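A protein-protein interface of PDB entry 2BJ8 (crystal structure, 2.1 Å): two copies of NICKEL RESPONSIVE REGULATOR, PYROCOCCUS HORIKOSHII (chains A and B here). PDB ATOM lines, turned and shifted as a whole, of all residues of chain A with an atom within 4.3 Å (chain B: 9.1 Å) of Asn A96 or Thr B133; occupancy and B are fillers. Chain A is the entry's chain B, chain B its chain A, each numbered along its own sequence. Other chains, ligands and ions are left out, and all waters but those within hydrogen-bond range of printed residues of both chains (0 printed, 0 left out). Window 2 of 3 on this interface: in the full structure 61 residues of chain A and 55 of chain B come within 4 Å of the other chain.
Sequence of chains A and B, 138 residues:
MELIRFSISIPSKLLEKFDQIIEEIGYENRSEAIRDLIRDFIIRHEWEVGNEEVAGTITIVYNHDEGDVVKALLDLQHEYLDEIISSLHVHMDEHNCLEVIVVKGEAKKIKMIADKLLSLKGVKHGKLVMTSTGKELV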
ATOM      1  N   VAL A  61       5.239 -22.346  11.719  1.00  0.00           N
ATOM      2  CA  VAL A  61       5.867 -21.035  11.778  1.00  0.00           C
ATOM      3  C   VAL A  61       5.661 -20.406  10.413  1.00  0.00           C
ATOM      4  O   VAL A  61       5.808 -21.073   9.388  1.00  0.00           O
ATOM      5  CB  VAL A  61       7.378 -21.120  12.062  1.00  0.00           C
ATOM      6  CG1 VAL A  61       7.990 -19.727  12.008  1.00  0.00           C
ATOM      7  CG2 VAL A  61       7.613 -21.734  13.436  1.00  0.00           C
ATOM      8  N   TYR A  62       5.312 -19.127  10.396  1.00  0.00           N
ATOM      9  CA  TYR A  62       5.077 -18.441   9.139  1.00  0.00           C
ATOM     10  C   TYR A  62       5.186 -16.936   9.290  1.00  0.00           C
ATOM     11  O   TYR A  62       5.168 -16.402  10.399  1.00  0.00           O
ATOM     12  CB  TYR A  62       3.686 -18.803   8.604  1.00  0.00           C
ATOM     13  CG  TYR A  62       2.555 -18.452   9.552  1.00  0.00           C
ATOM     14  CD1 TYR A  62       2.045 -17.152   9.619  1.00  0.00           C
ATOM     15  CD2 TYR A  62       2.014 -19.414  10.404  1.00  0.00           C
ATOM     16  CE1 TYR A  62       1.027 -16.823  10.510  1.00  0.00           C
ATOM     17  CE2 TYR A  62       0.997 -19.092  11.303  1.00  0.00           C
ATOM     18  CZ  TYR A  62       0.508 -17.799  11.350  1.00  0.00           C
ATOM     19  OH  TYR A  62      -0.495 -17.485  12.240  1.00  0.00           O
ATOM     20  N   ASN A  63       5.313 -16.265   8.154  1.00  0.00           N
ATOM     21  CA  ASN A  63       5.393 -14.814   8.100  1.00  0.00           C
ATOM     22  C   ASN A  63       3.969 -14.400   7.745  1.00  0.00           C
ATOM     23  O   ASN A  63       3.508 -14.671   6.635  1.00  0.00           O
ATOM     24  CB  ASN A  63       6.358 -14.393   6.989  1.00  0.00           C
ATOM     25  CG  ASN A  63       6.452 -12.887   6.833  1.00  0.00           C
ATOM     26  OD1 ASN A  63       5.442 -12.203   6.658  1.00  0.00           O
ATOM     27  ND2 ASN A  63       7.671 -12.364   6.888  1.00  0.00           N
ATOM     28  N   HIS A  91       3.762 -14.140  18.777  1.00  0.00           N
ATOM     29  CA  HIS A  91       4.371 -13.255  17.786  1.00  0.00           C
ATOM     30  C   HIS A  91       5.872 -13.234  18.047  1.00  0.00           C
ATOM     31  O   HIS A  91       6.339 -12.612  19.001  1.00  0.00           O
ATOM     32  CB  HIS A  91       3.777 -11.852  17.903  1.00  0.00           C
ATOM     33  CG  HIS A  91       2.280 -11.839  17.888  1.00  0.00           C
ATOM     34  ND1 HIS A  91       1.543 -12.425  16.881  1.00  0.00           N
ATOM     35  CD2 HIS A  91       1.382 -11.341  18.770  1.00  0.00           C
ATOM     36  CE1 HIS A  91       0.256 -12.289  17.142  1.00  0.00           C
ATOM     37  NE2 HIS A  91       0.130 -11.635  18.283  1.00  0.00           N
ATOM     38  N   MET A  92       6.609 -13.937  17.190  1.00  0.00           N
ATOM     39  CA  MET A  92       8.064 -14.081  17.286  1.00  0.00           C
ATOM     40  C   MET A  92       8.827 -12.785  17.058  1.00  0.00           C
ATOM     41  O   MET A  92       9.683 -12.404  17.853  1.00  0.00           O
ATOM     42  CB  MET A  92       8.529 -15.127  16.276  1.00  0.00           C
ATOM     43  CG  MET A  92       7.930 -16.508  16.495  1.00  0.00           C
ATOM     44  SD  MET A  92       8.725 -17.408  17.841  1.00  0.00           S
ATOM     45  CE  MET A  92       7.958 -16.685  19.253  1.00  0.00           C
ATOM     46  N   ASP A  93       8.531 -12.126  15.947  1.00  0.00           N
ATOM     47  CA  ASP A  93       9.165 -10.861  15.613  1.00  0.00           C
ATOM     48  C   ASP A  93       8.184 -10.088  14.748  1.00  0.00           C
ATOM     49  O   ASP A  93       7.046 -10.517  14.553  1.00  0.00           O
ATOM     50  CB  ASP A  93      10.490 -11.081  14.864  1.00  0.00           C
ATOM     51  CG  ASP A  93      10.329 -11.933  13.621  1.00  0.00           C
ATOM     52  OD1 ASP A  93       9.533 -11.559  12.730  1.00  0.00           O
ATOM     53  OD2 ASP A  93      11.004 -12.978  13.533  1.00  0.00           O
ATOM     54  N   GLU A  94       8.624  -8.953  14.224  1.00  0.00           N
ATOM     55  CA  GLU A  94       7.758  -8.130  13.408  1.00  0.00           C
ATOM     56  C   GLU A  94       7.021  -8.900  12.321  1.00  0.00           C
ATOM     57  O   GLU A  94       5.878  -8.580  11.999  1.00  0.00           O
ATOM     58  CB  GLU A  94       8.557  -6.999  12.763  1.00  0.00           C
ATOM     59  CG  GLU A  94       7.728  -6.132  11.827  1.00  0.00           C
ATOM     60  CD  GLU A  94       8.549  -5.078  11.114  1.00  0.00           C
ATOM     61  OE1 GLU A  94       7.971  -4.339  10.287  1.00  0.00           O
ATOM     62  OE2 GLU A  94       9.769  -4.987  11.376  1.00  0.00           O
ATOM     63  N   HIS A  95       7.660  -9.923  11.766  1.00  0.00           N
ATOM     64  CA  HIS A  95       7.045 -10.680  10.682  1.00  0.00           C
ATOM     65  C   HIS A  95       6.686 -12.139  10.945  1.00  0.00           C
ATOM     66  O   HIS A  95       5.747 -12.662  10.344  1.00  0.00           O
ATOM     67  CB  HIS A  95       7.943 -10.616   9.444  1.00  0.00           C
ATOM     68  CG  HIS A  95       8.108  -9.236   8.885  1.00  0.00           C
ATOM     69  ND1 HIS A  95       7.043  -8.487   8.432  1.00  0.00           N
ATOM     70  CD2 HIS A  95       9.210  -8.471   8.706  1.00  0.00           C
ATOM     71  CE1 HIS A  95       7.483  -7.320   7.995  1.00  0.00           C
ATOM     72  NE2 HIS A  95       8.795  -7.285   8.151  1.00  0.00           N
ATOM     73  N   ASN A  96       7.417 -12.796  11.835  1.00  0.00           N
ATOM     74  CA  ASN A  96       7.161 -14.204  12.095  1.00  0.00           C
ATOM     75  C   ASN A  96       6.262 -14.559  13.276  1.00  0.00           C
ATOM     76  O   ASN A  96       6.384 -14.006  14.371  1.00  0.00           O
ATOM     77  CB  ASN A  96       8.494 -14.939  12.219  1.00  0.00           C
ATOM     78  CG  ASN A  96       9.308 -14.865  10.944  1.00  0.00           C
ATOM     79  OD1 ASN A  96       8.865 -15.306   9.886  1.00  0.00           O
ATOM     80  ND2 ASN A  96      10.501 -14.294  11.036  1.00  0.00           N
ATOM     81  N   CYS A  97       5.363 -15.505  13.021  1.00  0.00           N
ATOM     82  CA  CYS A  97       4.417 -16.001  14.009  1.00  0.00           C
ATOM     83  C   CYS A  97       4.634 -17.490  14.233  1.00  0.00           C
ATOM     84  O   CYS A  97       4.985 -18.228  13.309  1.00  0.00           O
ATOM     85  CB  CYS A  97       2.976 -15.816  13.519  1.00  0.00           C
ATOM     86  SG  CYS A  97       2.439 -14.127  13.179  1.00  0.00           S
ATOM     87  N   LYS A 124       6.568 -22.082   6.764  1.00  0.00           N
ATOM     88  CA  LYS A 124       8.008 -22.294   6.645  1.00  0.00           C
ATOM     89  C   LYS A 124       8.496 -23.544   7.361  1.00  0.00           C
ATOM     90  O   LYS A 124       9.360 -24.262   6.861  1.00  0.00           O
ATOM     91  CB  LYS A 124       8.764 -21.091   7.212  1.00  0.00           C
ATOM     92  CG  LYS A 124       8.418 -19.750   6.591  1.00  0.00           C
ATOM     93  CD  LYS A 124       9.241 -18.650   7.260  1.00  0.00           C
ATOM     94  CE  LYS A 124       8.993 -17.281   6.648  1.00  0.00           C
ATOM     95  NZ  LYS A 124       9.889 -16.258   7.261  1.00  0.00           N
ATOM     96  N   GLU B  52      21.949 -22.391  18.462  1.00  0.00           N
ATOM     97  CA  GLU B  52      21.305 -21.228  17.883  1.00  0.00           C
ATOM     98  C   GLU B  52      20.034 -20.920  18.660  1.00  0.00           C
ATOM     99  O   GLU B  52      19.699 -21.602  19.632  1.00  0.00           O
ATOM    100  CB  GLU B  52      20.965 -21.488  16.414  1.00  0.00           C
ATOM    101  CG  GLU B  52      22.172 -21.508  15.492  1.00  0.00           C
ATOM    102  CD  GLU B  52      21.815 -21.910  14.072  1.00  0.00           C
ATOM    103  OE1 GLU B  52      20.832 -21.364  13.527  1.00  0.00           O
ATOM    104  OE2 GLU B  52      22.523 -22.767  13.501  1.00  0.00           O
ATOM    105  N   GLU B  53      19.332 -19.881  18.232  1.00  0.00           N
ATOM    106  CA  GLU B  53      18.092 -19.497  18.873  1.00  0.00           C
ATOM    107  C   GLU B  53      16.958 -20.264  18.226  1.00  0.00           C
ATOM    108  O   GLU B  53      16.809 -20.259  17.004  1.00  0.00           O
ATOM    109  CB  GLU B  53      17.870 -17.993  18.719  1.00  0.00           C
ATOM    110  CG  GLU B  53      18.573 -17.177  19.782  1.00  0.00           C
ATOM    111  CD  GLU B  53      17.834 -17.210  21.102  1.00  0.00           C
ATOM    112  OE1 GLU B  53      18.483 -17.061  22.160  1.00  0.00           O
ATOM    113  OE2 GLU B  53      16.596 -17.373  21.077  1.00  0.00           O
ATOM    114  N   VAL B  54      16.164 -20.940  19.047  1.00  0.00           N
ATOM    115  CA  VAL B  54      15.043 -21.703  18.525  1.00  0.00           C
ATOM    116  C   VAL B  54      13.766 -21.393  19.284  1.00  0.00           C
ATOM    117  O   VAL B  54      13.797 -20.883  20.402  1.00  0.00           O
ATOM    118  CB  VAL B  54      15.299 -23.228  18.599  1.00  0.00           C
ATOM    119  CG1 VAL B  54      16.519 -23.591  17.772  1.00  0.00           C
ATOM    120  CG2 VAL B  54      15.483 -23.663  20.048  1.00  0.00           C
ATOM    121  N   ALA B  55      12.646 -21.695  18.642  1.00  0.00           N
ATOM    122  CA  ALA B  55      11.328 -21.498  19.215  1.00  0.00           C
ATOM    123  C   ALA B  55      10.681 -22.866  19.108  1.00  0.00           C
ATOM    124  O   ALA B  55      10.736 -23.495  18.052  1.00  0.00           O
ATOM    125  CB  ALA B  55      10.548 -20.485  18.402  1.00  0.00           C
ATOM    126  N   GLY B  56      10.079 -23.341  20.189  1.00  0.00           N
ATOM    127  CA  GLY B  56       9.467 -24.651  20.120  1.00  0.00           C
ATOM    128  C   GLY B  56       8.213 -24.871  20.934  1.00  0.00           C
ATOM    129  O   GLY B  56       7.661 -23.952  21.538  1.00  0.00           O
ATOM    130  N   ILE B  85       7.229 -19.256  27.387  1.00  0.00           N
ATOM    131  CA  ILE B  85       6.354 -18.144  27.034  1.00  0.00           C
ATOM    132  C   ILE B  85       4.945 -18.267  27.609  1.00  0.00           C
ATOM    133  O   ILE B  85       4.473 -17.364  28.296  1.00  0.00           O
ATOM    134  CB  ILE B  85       6.232 -18.015  25.500  1.00  0.00           C
ATOM    135  CG1 ILE B  85       7.613 -17.786  24.888  1.00  0.00           C
ATOM    136  CG2 ILE B  85       5.299 -16.869  25.144  1.00  0.00           C
ATOM    137  CD1 ILE B  85       7.613 -17.771  23.376  1.00  0.00           C
ATOM    138  N   VAL B 103       8.091 -22.527  23.972  1.00  0.00           N
ATOM    139  CA  VAL B 103       9.378 -22.060  24.481  1.00  0.00           C
ATOM    140  C   VAL B 103      10.252 -21.382  23.429  1.00  0.00           C
ATOM    141  O   VAL B 103      10.078 -21.583  22.222  1.00  0.00           O
ATOM    142  CB  VAL B 103      10.187 -23.228  25.064  1.00  0.00           C
ATOM    143  CG1 VAL B 103       9.438 -23.857  26.224  1.00  0.00           C
ATOM    144  CG2 VAL B 103      10.442 -24.260  23.981  1.00  0.00           C
ATOM    145  N   LYS B 104      11.195 -20.574  23.903  1.00  0.00           N
ATOM    146  CA  LYS B 104      12.126 -19.877  23.022  1.00  0.00           C
ATOM    147  C   LYS B 104      13.446 -19.705  23.763  1.00  0.00           C
ATOM    148  O   LYS B 104      13.462 -19.416  24.958  1.00  0.00           O
ATOM    149  CB  LYS B 104      11.573 -18.507  22.610  1.00  0.00           C
ATOM    150  CG  LYS B 104      11.403 -17.526  23.756  1.00  0.00           C
ATOM    151  CD  LYS B 104      10.862 -16.179  23.279  1.00  0.00           C
ATOM    152  CE  LYS B 104      10.703 -15.206  24.449  1.00  0.00           C
ATOM    153  NZ  LYS B 104      10.140 -13.884  24.043  1.00  0.00           N
ATOM    154  N   GLY B 105      14.550 -19.901  23.052  1.00  0.00           N
ATOM    155  CA  GLY B 105      15.855 -19.760  23.671  1.00  0.00           C
ATOM    156  C   GLY B 105      16.918 -20.527  22.908  1.00  0.00           C
ATOM    157  O   GLY B 105      16.719 -20.895  21.747  1.00  0.00           O
ATOM    158  N   MET B 130      11.345 -28.439  17.903  1.00  0.00           N
ATOM    159  CA  MET B 130      12.191 -27.246  17.850  1.00  0.00           C
ATOM    160  C   MET B 130      12.302 -26.795  16.411  1.00  0.00           C
ATOM    161  O   MET B 130      12.404 -27.612  15.499  1.00  0.00           O
ATOM    162  CB  MET B 130      13.602 -27.522  18.373  1.00  0.00           C
ATOM    163  CG  MET B 130      13.735 -27.610  19.879  1.00  0.00           C
ATOM    164  SD  MET B 130      15.471 -27.543  20.385  1.00  0.00           S
ATOM    165  CE  MET B 130      15.980 -29.222  20.072  1.00  0.00           C
ATOM    166  N   THR B 131      12.295 -25.488  16.205  1.00  0.00           N
ATOM    167  CA  THR B 131      12.395 -24.952  14.863  1.00  0.00           C
ATOM    168  C   THR B 131      13.078 -23.596  14.902  1.00  0.00           C
ATOM    169  O   THR B 131      13.131 -22.947  15.948  1.00  0.00           O
ATOM    170  CB  THR B 131      10.990 -24.814  14.224  1.00  0.00           C
ATOM    171  OG1 THR B 131      11.098 -24.162  12.953  1.00  0.00           O
ATOM    172  CG2 THR B 131      10.062 -24.014  15.129  1.00  0.00           C
ATOM    173  N   SER B 132      13.627 -23.185  13.764  1.00  0.00           N
ATOM    174  CA  SER B 132      14.283 -21.892  13.659  1.00  0.00           C
ATOM    175  C   SER B 132      13.301 -20.978  12.947  1.00  0.00           C
ATOM    176  O   SER B 132      12.931 -21.238  11.805  1.00  0.00           O
ATOM    177  CB  SER B 132      15.570 -22.008  12.844  1.00  0.00           C
ATOM    178  OG  SER B 132      16.249 -20.765  12.793  1.00  0.00           O
ATOM    179  N   THR B 133      12.874 -19.915  13.622  1.00  0.00           N
ATOM    180  CA  THR B 133      11.918 -18.970  13.049  1.00  0.00           C
ATOM    181  C   THR B 133      12.371 -18.372  11.715  1.00  0.00           C
ATOM    182  O   THR B 133      11.678 -17.532  11.139  1.00  0.00           O
ATOM    183  CB  THR B 133      11.632 -17.815  14.031  1.00  0.00           C
ATOM    184  OG1 THR B 133      12.844 -17.099  14.298  1.00  0.00           O
ATOM    185  CG2 THR B 133      11.073 -18.357  15.340  1.00  0.00           C
ATOM    186  N   GLY B 134      13.528 -18.812  11.227  1.00  0.00           N
ATOM    187  CA  GLY B 134      14.054 -18.305   9.971  1.00  0.00           C
ATOM    188  C   GLY B 134      13.291 -18.745   8.733  1.00  0.00           C
ATOM    189  O   GLY B 134      12.073 -18.926   8.767  1.00  0.00           O
ATOM    190  N   LYS B 135      14.020 -18.915   7.634  1.00  0.00           N
ATOM    191  CA  LYS B 135      13.427 -19.330   6.368  1.00  0.00           C
ATOM    192  C   LYS B 135      13.404 -20.851   6.257  1.00  0.00           C
ATOM    193  O   LYS B 135      14.220 -21.539   6.874  1.00  0.00           O
ATOM    194  CB  LYS B 135      14.220 -18.727   5.207  1.00  0.00           C
ATOM    195  CG  LYS B 135      14.305 -17.210   5.268  1.00  0.00           C
ATOM    196  CD  LYS B 135      15.202 -16.645   4.182  1.00  0.00           C
ATOM    197  CE  LYS B 135      15.319 -15.134   4.311  1.00  0.00           C
ATOM    198  NZ  LYS B 135      16.236 -14.556   3.290  1.00  0.00           N
ATOM    199  N   GLU B 136      12.469 -21.367   5.464  1.00  0.00           N
ATOM    200  CA  GLU B 136      12.306 -22.809   5.278  1.00  0.00           C
ATOM    201  C   GLU B 136      13.618 -23.541   4.985  1.00  0.00           C
ATOM    202  O   GLU B 136      14.632 -22.869   4.704  1.00  0.00           O
ATOM    203  CB  GLU B 136      11.309 -23.076   4.146  1.00  0.00           C
ATOM    204  CG  GLU B 136      10.749 -24.491   4.133  1.00  0.00           C
ATOM    205  CD  GLU B 136       9.829 -24.748   2.952  1.00  0.00           C
ATOM    206  OE1 GLU B 136       8.982 -23.878   2.650  1.00  0.00           O
ATOM    207  OE2 GLU B 136       9.945 -25.826   2.331  1.00  0.00           O
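No position is printed for both chains.
Of the 6 pairs that touch across the chains among the printed residues, none has its exchanged pair printed and touching as well.
Among the printed residues, merely in contact across the chains: Lys A124 with Glu B136, Lys A124 with Gly B134, Met A92 with Thr B133, Met A92 with Ala B55 and Val A61 with Thr B131.
O of Thr B133 is in hydrogen-bond range of ND2 of Asn A96, 3.4 Å away.
The backbone NH (N) of Ala B55 sits at hydrogen-bond distance from the backbone carbonyl oxygen (O) of Thr B131 (3.0 Å).
O of Val A61 sits at hydrogen-bond distance from N of Lys A124, 2.9 Å away.
The side-chain carboxylate of Asp A93 lies within hydrogen-bond range of the backbone NH of Asn A96 (2.6 Å).
The side-chain amide oxygen (OD1) of Asn A96 sits at hydrogen-bond distance from the side-chain amino group (NZ) of Lys A124, 3.0 Å away.
Of the 16 printed residues of chain B, 5 touch a printed residue of chain A.
Among the printed residues, no Asp or Glu carboxylate lies within 4 Å of a Lys or Arg side-chain nitrogen of the other chain.
Thr B133 touches just these residues of chain A: Met A92 and Asn A96.
No residue of chain B comes within 4 Å of Asp A93.
No residue of chain B comes within 4 Å of Cys A97.
Printed residues of chain A within 4 Å of Thr B131: Val A61.
Of the printed residues of chain B, Val A61 touches Thr B131 (3.7 Å).
Val B103 touches none of the printed residues of chain A.
The nearest residue of chain B that does not touch Asn A96 is Gly B134 (5.0 Å).
The nearest printed residue of chain A that does not touch Glu B136 is Val A61 (7.7 Å).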
